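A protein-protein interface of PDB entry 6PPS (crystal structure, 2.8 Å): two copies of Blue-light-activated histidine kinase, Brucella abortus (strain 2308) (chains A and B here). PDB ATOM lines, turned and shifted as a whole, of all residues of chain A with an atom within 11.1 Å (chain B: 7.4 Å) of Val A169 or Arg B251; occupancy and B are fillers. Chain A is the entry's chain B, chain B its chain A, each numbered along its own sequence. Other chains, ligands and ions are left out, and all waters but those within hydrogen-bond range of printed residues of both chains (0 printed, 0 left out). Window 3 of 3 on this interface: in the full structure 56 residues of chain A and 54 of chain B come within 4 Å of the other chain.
Ile A172 touches its own counterpart, Ile B172. Positions printed for both chains: 172, 173 and 174.
Gln A162 touches Phe B174 (OE1 to CE2, 3.5 Å). Gln A162 touches Leu B263 (CG to CD2, 3.6 Å). Ala B252 touches Tyr A165 (CA to OH, 3.6 Å). Tyr A165 touches Lys B253 (CE1 to CB, 3.7 Å). Ile A166 touches Ile B172. Phe B174 touches Ile A166. Val A169 touches Arg B251 (CG1 to CZ, 3.5 Å). Ile B172 touches Ala A170 (CD1 to CB, 3.6 Å). CD1 of Ile B172 touches CD1 of Ile A172, 3.5 Å away.
O of Arg B251 sits at hydrogen-bond distance from OH of Tyr A165, 2.7 Å away.
Printed residues of chain B within 4 Å of Ile A166: Ile B172 and Phe B174. Val A169 touches one residue of chain B. Printed residues of chain B within 4 Å of Ala A170: Ile B172 (3.6 Å). Printed residues of chain A within 4 Å of Phe B174: Gln A162 and Ile A166. Trp B175 touches none of the printed residues of chain A. No residue of chain A comes within 4 Å of Ser B233. No residue of chain A comes within 4 Å of Thr B250. Of chain A, only Tyr A165 and Val A169 come within 4 Å of Arg B251. Printed residues of chain A within 4 Å of Ala B252: Tyr A165. Printed residues of chain A within 4 Å of Leu B263: Gln A162. No residue of chain A comes within 4 Å of Gly B264. The nearest residue of chain B that does not touch Val A169 is Ile B265 (4.2 Å).
Printed residues of chain B that touch a printed residue of chain A: Ile B172, Phe B174, Arg B251, Ala B252, Lys B253 and Leu B263. Of the 18 printed residues of chain A, 6 touch a printed residue of chain B. Hydrophobic or aromatic side chains of chain A within 4 Å of the printed part of chain B: Tyr A165, Ile A166, Val A169, Ala A170 and Ile A172. Among the printed residues, 10 pairs touch across the chains.
The backbone carbonyl oxygen of Tyr B232 lies within hydrogen-bond range of the backbone NH of Ala B252 (2.8 Å). The backbone NH (N) of Ile B265 lies within hydrogen-bond range of the backbone carbonyl oxygen (O) of Arg B251, 3.2 Å away. N of Leu B263 lies within hydrogen-bond range of O of Lys B253. O of Val A167 is in hydrogen-bond range of N of Ile A172. The backbone carbonyl oxygen (O) of Ile A172 sits at hydrogen-bond distance from the side-chain hydroxyl (OG) of Ser A187 (2.7 Å).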
ATOM      1  N   ASP A 161      19.289 -14.404  30.522  1.00  0.00           N
ATOM      2  CA  ASP A 161      17.901 -14.171  30.136  1.00  0.00           C
ATOM      3  C   ASP A 161      17.478 -15.142  29.039  1.00  0.00           C
ATOM      4  O   ASP A 161      16.319 -15.553  28.975  1.00  0.00           O
ATOM      5  CB  ASP A 161      17.705 -12.727  29.662  1.00  0.00           C
ATOM      6  CG  ASP A 161      17.598 -11.742  30.811  1.00  0.00           C
ATOM      7  OD1 ASP A 161      17.972 -12.105  31.947  1.00  0.00           O
ATOM      8  OD2 ASP A 161      17.143 -10.602  30.576  1.00  0.00           O
ATOM      9  N   GLN A 162      18.425 -15.502  28.178  1.00  0.00           N
ATOM     10  CA  GLN A 162      18.159 -16.427  27.081  1.00  0.00           C
ATOM     11  C   GLN A 162      17.928 -17.844  27.594  1.00  0.00           C
ATOM     12  O   GLN A 162      17.041 -18.550  27.116  1.00  0.00           O
ATOM     13  CB  GLN A 162      19.314 -16.418  26.075  1.00  0.00           C
ATOM     14  CG  GLN A 162      19.524 -15.087  25.371  1.00  0.00           C
ATOM     15  CD  GLN A 162      20.678 -15.117  24.388  1.00  0.00           C
ATOM     16  OE1 GLN A 162      20.818 -16.056  23.603  1.00  0.00           O
ATOM     17  NE2 GLN A 162      21.516 -14.088  24.429  1.00  0.00           N
ATOM     18  N   LEU A 163      18.736 -18.249  28.571  1.00  0.00           N
ATOM     19  CA  LEU A 163      18.669 -19.595  29.133  1.00  0.00           C
ATOM     20  C   LEU A 163      17.308 -19.893  29.753  1.00  0.00           C
ATOM     21  O   LEU A 163      16.678 -20.901  29.436  1.00  0.00           O
ATOM     22  CB  LEU A 163      19.763 -19.791  30.185  1.00  0.00           C
ATOM     23  CG  LEU A 163      19.856 -21.189  30.800  1.00  0.00           C
ATOM     24  CD1 LEU A 163      20.521 -22.153  29.831  1.00  0.00           C
ATOM     25  CD2 LEU A 163      20.596 -21.154  32.126  1.00  0.00           C
ATOM     26  N   ASP A 164      16.864 -19.008  30.641  1.00  0.00           N
ATOM     27  CA  ASP A 164      15.604 -19.197  31.349  1.00  0.00           C
ATOM     28  C   ASP A 164      14.409 -19.133  30.405  1.00  0.00           C
ATOM     29  O   ASP A 164      13.394 -19.793  30.633  1.00  0.00           O
ATOM     30  CB  ASP A 164      15.453 -18.151  32.456  1.00  0.00           C
ATOM     31  CG  ASP A 164      16.535 -18.263  33.511  1.00  0.00           C
ATOM     32  OD1 ASP A 164      17.095 -19.367  33.677  1.00  0.00           O
ATOM     33  OD2 ASP A 164      16.825 -17.246  34.177  1.00  0.00           O
ATOM     34  N   TYR A 165      14.533 -18.339  29.347  1.00  0.00           N
ATOM     35  CA  TYR A 165      13.467 -18.218  28.362  1.00  0.00           C
ATOM     36  C   TYR A 165      13.278 -19.523  27.595  1.00  0.00           C
ATOM     37  O   TYR A 165      12.153 -19.969  27.382  1.00  0.00           O
ATOM     38  CB  TYR A 165      13.752 -17.075  27.385  1.00  0.00           C
ATOM     39  CG  TYR A 165      12.794 -17.031  26.216  1.00  0.00           C
ATOM     40  CD1 TYR A 165      11.533 -16.463  26.347  1.00  0.00           C
ATOM     41  CD2 TYR A 165      13.148 -17.559  24.980  1.00  0.00           C
ATOM     42  CE1 TYR A 165      10.652 -16.423  25.282  1.00  0.00           C
ATOM     43  CE2 TYR A 165      12.275 -17.525  23.912  1.00  0.00           C
ATOM     44  CZ  TYR A 165      11.028 -16.956  24.068  1.00  0.00           C
ATOM     45  OH  TYR A 165      10.156 -16.919  23.004  1.00  0.00           O
ATOM     46  N   ILE A 166      14.386 -20.128  27.182  1.00  0.00           N
ATOM     47  CA  ILE A 166      14.341 -21.365  26.410  1.00  0.00           C
ATOM     48  C   ILE A 166      13.786 -22.527  27.230  1.00  0.00           C
ATOM     49  O   ILE A 166      12.906 -23.256  26.771  1.00  0.00           O
ATOM     50  CB  ILE A 166      15.734 -21.744  25.879  1.00  0.00           C
ATOM     51  CG1 ILE A 166      16.175 -20.753  24.803  1.00  0.00           C
ATOM     52  CG2 ILE A 166      15.730 -23.152  25.314  1.00  0.00           C
ATOM     53  CD1 ILE A 166      17.468 -21.133  24.129  1.00  0.00           C
ATOM     54  N   VAL A 167      14.303 -22.686  28.443  1.00  0.00           N
ATOM     55  CA  VAL A 167      13.884 -23.765  29.332  1.00  0.00           C
ATOM     56  C   VAL A 167      12.386 -23.703  29.639  1.00  0.00           C
ATOM     57  O   VAL A 167      11.697 -24.725  29.629  1.00  0.00           O
ATOM     58  CB  VAL A 167      14.678 -23.734  30.655  1.00  0.00           C
ATOM     59  CG1 VAL A 167      14.134 -24.758  31.633  1.00  0.00           C
ATOM     60  CG2 VAL A 167      16.153 -23.985  30.389  1.00  0.00           C
ATOM     61  N   GLU A 168      11.886 -22.499  29.897  1.00  0.00           N
ATOM     62  CA  GLU A 168      10.479 -22.312  30.232  1.00  0.00           C
ATOM     63  C   GLU A 168       9.566 -22.576  29.039  1.00  0.00           C
ATOM     64  O   GLU A 168       8.631 -23.374  29.124  1.00  0.00           O
ATOM     65  CB  GLU A 168      10.240 -20.896  30.761  1.00  0.00           C
ATOM     66  CG  GLU A 168       8.790 -20.611  31.116  1.00  0.00           C
ATOM     67  CD  GLU A 168       8.555 -19.166  31.508  1.00  0.00           C
ATOM     68  OE1 GLU A 168       7.459 -18.861  32.023  1.00  0.00           O
ATOM     69  OE2 GLU A 168       9.462 -18.334  31.297  1.00  0.00           O
ATOM     70  N   VAL A 169       9.845 -21.901  27.928  1.00  0.00           N
ATOM     71  CA  VAL A 169       9.002 -21.971  26.738  1.00  0.00           C
ATOM     72  C   VAL A 169       9.001 -23.359  26.095  1.00  0.00           C
ATOM     73  O   VAL A 169       7.967 -23.827  25.611  1.00  0.00           O
ATOM     74  CB  VAL A 169       9.446 -20.919  25.693  1.00  0.00           C
ATOM     75  CG1 VAL A 169       8.715 -21.112  24.373  1.00  0.00           C
ATOM     76  CG2 VAL A 169       9.216 -19.516  26.231  1.00  0.00           C
ATOM     77  N   ALA A 170      10.152 -24.024  26.106  1.00  0.00           N
ATOM     78  CA  ALA A 170      10.288 -25.308  25.423  1.00  0.00           C
ATOM     79  C   ALA A 170      10.036 -26.506  26.340  1.00  0.00           C
ATOM     80  O   ALA A 170      10.200 -27.651  25.918  1.00  0.00           O
ATOM     81  CB  ALA A 170      11.664 -25.417  24.791  1.00  0.00           C
ATOM     82  N   ASN A 171       9.633 -26.234  27.580  1.00  0.00           N
ATOM     83  CA  ASN A 171       9.326 -27.277  28.562  1.00  0.00           C
ATOM     84  C   ASN A 171      10.416 -28.340  28.677  1.00  0.00           C
ATOM     85  O   ASN A 171      10.174 -29.519  28.418  1.00  0.00           O
ATOM     86  CB  ASN A 171       7.990 -27.951  28.224  1.00  0.00           C
ATOM     87  CG  ASN A 171       6.795 -27.080  28.564  1.00  0.00           C
ATOM     88  OD1 ASN A 171       6.823 -26.317  29.530  1.00  0.00           O
ATOM     89  ND2 ASN A 171       5.734 -27.192  27.770  1.00  0.00           N
ATOM     90  N   ILE A 172      11.613 -27.918  29.070  1.00  0.00           N
ATOM     91  CA  ILE A 172      12.752 -28.825  29.150  1.00  0.00           C
ATOM     92  C   ILE A 172      13.072 -29.243  30.580  1.00  0.00           C
ATOM     93  O   ILE A 172      13.165 -28.406  31.478  1.00  0.00           O
ATOM     94  CB  ILE A 172      14.013 -28.191  28.536  1.00  0.00           C
ATOM     95  CG1 ILE A 172      13.795 -27.899  27.054  1.00  0.00           C
ATOM     96  CG2 ILE A 172      15.219 -29.100  28.717  1.00  0.00           C
ATOM     97  CD1 ILE A 172      15.045 -27.451  26.356  1.00  0.00           C
ATOM     98  N   GLY A 173      13.237 -30.546  30.782  1.00  0.00           N
ATOM     99  CA  GLY A 173      13.712 -31.064  32.049  1.00  0.00           C
ATOM    100  C   GLY A 173      15.207 -30.854  32.167  1.00  0.00           C
ATOM    101  O   GLY A 173      15.998 -31.754  31.886  1.00  0.00           O
ATOM    102  N   PHE A 174      15.597 -29.653  32.581  1.00  0.00           N
ATOM    103  CA  PHE A 174      17.006 -29.292  32.655  1.00  0.00           C
ATOM    104  C   PHE A 174      17.489 -29.179  34.094  1.00  0.00           C
ATOM    105  O   PHE A 174      16.817 -28.588  34.939  1.00  0.00           O
ATOM    106  CB  PHE A 174      17.250 -27.975  31.919  1.00  0.00           C
ATOM    107  CG  PHE A 174      18.666 -27.484  32.008  1.00  0.00           C
ATOM    108  CD1 PHE A 174      19.695 -28.187  31.403  1.00  0.00           C
ATOM    109  CD2 PHE A 174      18.965 -26.315  32.685  1.00  0.00           C
ATOM    110  CE1 PHE A 174      20.999 -27.736  31.478  1.00  0.00           C
ATOM    111  CE2 PHE A 174      20.267 -25.856  32.764  1.00  0.00           C
ATOM    112  CZ  PHE A 174      21.285 -26.568  32.159  1.00  0.00           C
ATOM    113  N   SER A 187      14.622 -27.382  36.795  1.00  0.00           N
ATOM    114  CA  SER A 187      13.564 -26.659  36.106  1.00  0.00           C
ATOM    115  C   SER A 187      12.203 -27.232  36.480  1.00  0.00           C
ATOM    116  O   SER A 187      12.118 -28.290  37.105  1.00  0.00           O
ATOM    117  CB  SER A 187      13.768 -26.724  34.593  1.00  0.00           C
ATOM    118  OG  SER A 187      13.745 -28.065  34.133  1.00  0.00           O
ATOM    119  N   ALA A 188      11.143 -26.533  36.091  1.00  0.00           N
ATOM    120  CA  ALA A 188       9.783 -26.955  36.408  1.00  0.00           C
ATOM    121  C   ALA A 188       9.447 -28.294  35.761  1.00  0.00           C
ATOM    122  O   ALA A 188       8.785 -29.137  36.366  1.00  0.00           O
ATOM    123  CB  ALA A 188       8.788 -25.893  35.975  1.00  0.00           C
ATOM    124  N   GLU A 189       9.908 -28.486  34.528  1.00  0.00           N
ATOM    125  CA  GLU A 189       9.668 -29.730  33.807  1.00  0.00           C
ATOM    126  C   GLU A 189      10.491 -30.869  34.397  1.00  0.00           C
ATOM    127  O   GLU A 189      10.047 -32.016  34.435  1.00  0.00           O
ATOM    128  CB  GLU A 189       9.987 -29.558  32.318  1.00  0.00           C
ATOM    129  CG  GLU A 189       9.920 -30.843  31.500  1.00  0.00           C
ATOM    130  CD  GLU A 189       8.523 -31.434  31.431  1.00  0.00           C
ATOM    131  OE1 GLU A 189       7.543 -30.697  31.674  1.00  0.00           O
ATOM    132  OE2 GLU A 189       8.403 -32.641  31.128  1.00  0.00           O
ATOM    133  N   ARG A 192       8.772 -32.146  37.489  1.00  0.00           N
ATOM    134  CA  ARG A 192       7.531 -32.836  37.164  1.00  0.00           C
ATOM    135  C   ARG A 192       7.809 -34.268  36.713  1.00  0.00           C
ATOM    136  O   ARG A 192       6.994 -35.165  36.928  1.00  0.00           O
ATOM    137  CB  ARG A 192       6.765 -32.067  36.083  1.00  0.00           C
ATOM    138  CG  ARG A 192       5.441 -32.690  35.670  1.00  0.00           C
ATOM    139  CD  ARG A 192       4.448 -31.637  35.186  1.00  0.00           C
ATOM    140  NE  ARG A 192       5.007 -30.759  34.160  1.00  0.00           N
ATOM    141  CZ  ARG A 192       5.426 -29.516  34.383  1.00  0.00           C
ATOM    142  NH1 ARG A 192       5.354 -28.998  35.602  1.00  0.00           N
ATOM    143  NH2 ARG A 192       5.920 -28.791  33.389  1.00  0.00           N
ATOM    144  N   ILE B 172      16.632 -27.550  19.475  1.00  0.00           N
ATOM    145  CA  ILE B 172      15.715 -26.421  19.442  1.00  0.00           C
ATOM    146  C   ILE B 172      16.123 -25.401  18.388  1.00  0.00           C
ATOM    147  O   ILE B 172      17.274 -24.968  18.342  1.00  0.00           O
ATOM    148  CB  ILE B 172      15.644 -25.719  20.809  1.00  0.00           C
ATOM    149  CG1 ILE B 172      15.097 -26.675  21.866  1.00  0.00           C
ATOM    150  CG2 ILE B 172      14.778 -24.473  20.729  1.00  0.00           C
ATOM    151  CD1 ILE B 172      14.869 -26.015  23.191  1.00  0.00           C
ATOM    152  N   GLY B 173      15.173 -25.024  17.538  1.00  0.00           N
ATOM    153  CA  GLY B 173      15.402 -23.969  16.570  1.00  0.00           C
ATOM    154  C   GLY B 173      15.416 -22.619  17.259  1.00  0.00           C
ATOM    155  O   GLY B 173      14.424 -21.894  17.253  1.00  0.00           O
ATOM    156  N   PHE B 174      16.551 -22.284  17.863  1.00  0.00           N
ATOM    157  CA  PHE B 174      16.679 -21.043  18.612  1.00  0.00           C
ATOM    158  C   PHE B 174      17.487 -20.007  17.842  1.00  0.00           C
ATOM    159  O   PHE B 174      18.556 -20.309  17.311  1.00  0.00           O
ATOM    160  CB  PHE B 174      17.328 -21.308  19.971  1.00  0.00           C
ATOM    161  CG  PHE B 174      17.569 -20.067  20.779  1.00  0.00           C
ATOM    162  CD1 PHE B 174      16.505 -19.331  21.276  1.00  0.00           C
ATOM    163  CD2 PHE B 174      18.859 -19.641  21.054  1.00  0.00           C
ATOM    164  CE1 PHE B 174      16.723 -18.190  22.026  1.00  0.00           C
ATOM    165  CE2 PHE B 174      19.084 -18.501  21.803  1.00  0.00           C
ATOM    166  CZ  PHE B 174      18.014 -17.774  22.290  1.00  0.00           C
ATOM    167  N   TRP B 175      16.967 -18.786  17.784  1.00  0.00           N
ATOM    168  CA  TRP B 175      17.672 -17.691  17.133  1.00  0.00           C
ATOM    169  C   TRP B 175      17.588 -16.403  17.944  1.00  0.00           C
ATOM    170  O   TRP B 175      16.649 -16.197  18.714  1.00  0.00           O
ATOM    171  CB  TRP B 175      17.124 -17.452  15.721  1.00  0.00           C
ATOM    172  CG  TRP B 175      15.645 -17.202  15.668  1.00  0.00           C
ATOM    173  CD1 TRP B 175      14.673 -18.115  15.384  1.00  0.00           C
ATOM    174  CD2 TRP B 175      14.971 -15.959  15.902  1.00  0.00           C
ATOM    175  NE1 TRP B 175      13.437 -17.520  15.427  1.00  0.00           N
ATOM    176  CE2 TRP B 175      13.592 -16.195  15.744  1.00  0.00           C
ATOM    177  CE3 TRP B 175      15.398 -14.668  16.230  1.00  0.00           C
ATOM    178  CZ2 TRP B 175      12.637 -15.194  15.903  1.00  0.00           C
ATOM    179  CZ3 TRP B 175      14.449 -13.675  16.390  1.00  0.00           C
ATOM    180  CH2 TRP B 175      13.085 -13.942  16.226  1.00  0.00           C
ATOM    181  N   PRO B 231       5.930 -11.591  25.237  1.00  0.00           N
ATOM    182  CA  PRO B 231       6.099 -12.658  24.248  1.00  0.00           C
ATOM    183  C   PRO B 231       5.024 -12.596  23.171  1.00  0.00           C
ATOM    184  O   PRO B 231       3.875 -12.267  23.469  1.00  0.00           O
ATOM    185  CB  PRO B 231       5.967 -13.934  25.084  1.00  0.00           C
ATOM    186  CG  PRO B 231       5.119 -13.533  26.241  1.00  0.00           C
ATOM    187  CD  PRO B 231       5.504 -12.113  26.547  1.00  0.00           C
ATOM    188  N   TYR B 232       5.393 -12.902  21.934  1.00  0.00           N
ATOM    189  CA  TYR B 232       4.434 -12.873  20.839  1.00  0.00           C
ATOM    190  C   TYR B 232       4.670 -14.019  19.862  1.00  0.00           C
ATOM    191  O   TYR B 232       5.795 -14.491  19.698  1.00  0.00           O
ATOM    192  CB  TYR B 232       4.495 -11.528  20.107  1.00  0.00           C
ATOM    193  CG  TYR B 232       5.820 -11.230  19.440  1.00  0.00           C
ATOM    194  CD1 TYR B 232       6.850 -10.613  20.139  1.00  0.00           C
ATOM    195  CD2 TYR B 232       6.037 -11.555  18.106  1.00  0.00           C
ATOM    196  CE1 TYR B 232       8.062 -10.336  19.530  1.00  0.00           C
ATOM    197  CE2 TYR B 232       7.243 -11.281  17.490  1.00  0.00           C
ATOM    198  CZ  TYR B 232       8.252 -10.671  18.206  1.00  0.00           C
ATOM    199  OH  TYR B 232       9.453 -10.400  17.593  1.00  0.00           O
ATOM    200  N   SER B 233       3.598 -14.467  19.219  1.00  0.00           N
ATOM    201  CA  SER B 233       3.691 -15.544  18.244  1.00  0.00           C
ATOM    202  C   SER B 233       3.478 -15.018  16.831  1.00  0.00           C
ATOM    203  O   SER B 233       2.697 -14.092  16.614  1.00  0.00           O
ATOM    204  CB  SER B 233       2.675 -16.644  18.557  1.00  0.00           C
ATOM    205  OG  SER B 233       2.944 -17.243  19.813  1.00  0.00           O
ATOM    206  N   ILE B 234       4.186 -15.610  15.877  1.00  0.00           N
ATOM    207  CA  ILE B 234       4.034 -15.247  14.476  1.00  0.00           C
ATOM    208  C   ILE B 234       4.275 -16.474  13.598  1.00  0.00           C
ATOM    209  O   ILE B 234       5.172 -17.278  13.857  1.00  0.00           O
ATOM    210  CB  ILE B 234       4.991 -14.095  14.079  1.00  0.00           C
ATOM    211  CG1 ILE B 234       4.749 -13.667  12.629  1.00  0.00           C
ATOM    212  CG2 ILE B 234       6.447 -14.484  14.310  1.00  0.00           C
ATOM    213  CD1 ILE B 234       5.530 -12.441  12.217  1.00  0.00           C
ATOM    214  N   GLU B 249       6.230 -21.786  12.673  1.00  0.00           N
ATOM    215  CA  GLU B 249       5.658 -21.082  13.815  1.00  0.00           C
ATOM    216  C   GLU B 249       6.782 -20.599  14.720  1.00  0.00           C
ATOM    217  O   GLU B 249       7.729 -21.339  14.989  1.00  0.00           O
ATOM    218  CB  GLU B 249       4.700 -21.981  14.598  1.00  0.00           C
ATOM    219  CG  GLU B 249       3.418 -22.333  13.868  1.00  0.00           C
ATOM    220  CD  GLU B 249       2.475 -23.156  14.726  1.00  0.00           C
ATOM    221  OE1 GLU B 249       2.698 -23.226  15.953  1.00  0.00           O
ATOM    222  OE2 GLU B 249       1.513 -23.733  14.174  1.00  0.00           O
ATOM    223  N   THR B 250       6.680 -19.362  15.194  1.00  0.00           N
ATOM    224  CA  THR B 250       7.732 -18.792  16.026  1.00  0.00           C
ATOM    225  C   THR B 250       7.176 -18.084  17.258  1.00  0.00           C
ATOM    226  O   THR B 250       6.281 -17.247  17.154  1.00  0.00           O
ATOM    227  CB  THR B 250       8.596 -17.793  15.230  1.00  0.00           C
ATOM    228  OG1 THR B 250       9.120 -18.435  14.061  1.00  0.00           O
ATOM    229  CG2 THR B 250       9.751 -17.290  16.082  1.00  0.00           C
ATOM    230  N   ARG B 251       7.713 -18.436  18.423  1.00  0.00           N
ATOM    231  CA  ARG B 251       7.381 -17.755  19.669  1.00  0.00           C
ATOM    232  C   ARG B 251       8.560 -16.888  20.091  1.00  0.00           C
ATOM    233  O   ARG B 251       9.620 -17.402  20.449  1.00  0.00           O
ATOM    234  CB  ARG B 251       7.028 -18.765  20.762  1.00  0.00           C
ATOM    235  CG  ARG B 251       5.755 -19.551  20.483  1.00  0.00           C
ATOM    236  CD  ARG B 251       5.564 -20.696  21.466  1.00  0.00           C
ATOM    237  NE  ARG B 251       5.476 -20.235  22.849  1.00  0.00           N
ATOM    238  CZ  ARG B 251       5.247 -21.033  23.886  1.00  0.00           C
ATOM    239  NH1 ARG B 251       5.081 -22.335  23.700  1.00  0.00           N
ATOM    240  NH2 ARG B 251       5.184 -20.530  25.112  1.00  0.00           N
ATOM    241  N   ALA B 252       8.377 -15.573  20.045  1.00  0.00           N
ATOM    242  CA  ALA B 252       9.491 -14.651  20.238  1.00  0.00           C
ATOM    243  C   ALA B 252       9.295 -13.685  21.405  1.00  0.00           C
ATOM    244  O   ALA B 252       8.176 -13.459  21.867  1.00  0.00           O
ATOM    245  CB  ALA B 252       9.742 -13.868  18.955  1.00  0.00           C
ATOM    246  N   LYS B 253      10.405 -13.119  21.870  1.00  0.00           N
ATOM    247  CA  LYS B 253      10.399 -12.137  22.949  1.00  0.00           C
ATOM    248  C   LYS B 253      11.604 -11.206  22.825  1.00  0.00           C
ATOM    249  O   LYS B 253      12.706 -11.647  22.499  1.00  0.00           O
ATOM    250  CB  LYS B 253      10.404 -12.830  24.315  1.00  0.00           C
ATOM    251  CG  LYS B 253      10.590 -11.876  25.489  1.00  0.00           C
ATOM    252  CD  LYS B 253      10.751 -12.613  26.807  1.00  0.00           C
ATOM    253  CE  LYS B 253       9.451 -13.268  27.240  1.00  0.00           C
ATOM    254  NZ  LYS B 253       9.576 -13.884  28.590  1.00  0.00           N
ATOM    255  N   LEU B 263      14.729 -12.547  21.067  1.00  0.00           N
ATOM    256  CA  LEU B 263      14.865 -13.994  21.189  1.00  0.00           C
ATOM    257  C   LEU B 263      13.705 -14.680  20.486  1.00  0.00           C
ATOM    258  O   LEU B 263      12.594 -14.157  20.473  1.00  0.00           O
ATOM    259  CB  LEU B 263      14.912 -14.413  22.658  1.00  0.00           C
ATOM    260  CG  LEU B 263      15.890 -13.641  23.541  1.00  0.00           C
ATOM    261  CD1 LEU B 263      15.898 -14.214  24.949  1.00  0.00           C
ATOM    262  CD2 LEU B 263      17.283 -13.659  22.933  1.00  0.00           C
ATOM    263  N   GLY B 264      13.956 -15.851  19.910  1.00  0.00           N
ATOM    264  CA  GLY B 264      12.915 -16.559  19.190  1.00  0.00           C
ATOM    265  C   GLY B 264      13.169 -18.038  18.978  1.00  0.00           C
ATOM    266  O   GLY B 264      14.283 -18.453  18.660  1.00  0.00           O
ATOM    267  N   ILE B 265      12.118 -18.832  19.154  1.00  0.00           N
ATOM    268  CA  ILE B 265      12.179 -20.268  18.918  1.00  0.00           C
ATOM    269  C   ILE B 265      11.244 -20.659  17.776  1.00  0.00           C
ATOM    270  O   ILE B 265      10.023 -20.560  17.899  1.00  0.00           O
ATOM    271  CB  ILE B 265      11.811 -21.064  20.184  1.00  0.00           C
ATOM    272  CG1 ILE B 265      12.813 -20.773  21.304  1.00  0.00           C
ATOM    273  CG2 ILE B 265      11.759 -22.551  19.882  1.00  0.00           C
ATOM    274  CD1 ILE B 265      12.543 -21.538  22.580  1.00  0.00           C
ATOM    275  N   VAL B 266      11.823 -21.098  16.663  1.00  0.00           N
ATOM    276  CA  VAL B 266      11.044 -21.456  15.484  1.00  0.00           C
ATOM    277  C   VAL B 266      10.956 -22.976  15.341  1.00  0.00           C
ATOM    278  O   VAL B 266      11.898 -23.695  15.676  1.00  0.00           O
ATOM    279  CB  VAL B 266      11.650 -20.833  14.201  1.00  0.00           C
ATOM    280  CG1 VAL B 266      13.046 -21.380  13.940  1.00  0.00           C
ATOM    281  CG2 VAL B 266      10.743 -21.062  12.996  1.00  0.00           C
ATOM    282  N   GLN B 267       9.814 -23.463  14.867  1.00  0.00           N
ATOM    283  CA  GLN B 267       9.630 -24.891  14.635  1.00  0.00           C
ATOM    284  C   GLN B 267       8.833 -25.147  13.357  1.00  0.00           C
ATOM    285  O   GLN B 267       7.921 -24.392  13.018  1.00  0.00           O
ATOM    286  CB  GLN B 267       8.941 -25.545  15.834  1.00  0.00           C
ATOM    287  CG  GLN B 267       7.667 -24.853  16.283  1.00  0.00           C
ATOM    288  CD  GLN B 267       7.033 -25.529  17.481  1.00  0.00           C
ATOM    289  OE1 GLN B 267       7.511 -26.562  17.949  1.00  0.00           O
ATOM    290  NE2 GLN B 267       5.951 -24.948  17.986  1.00  0.00           N
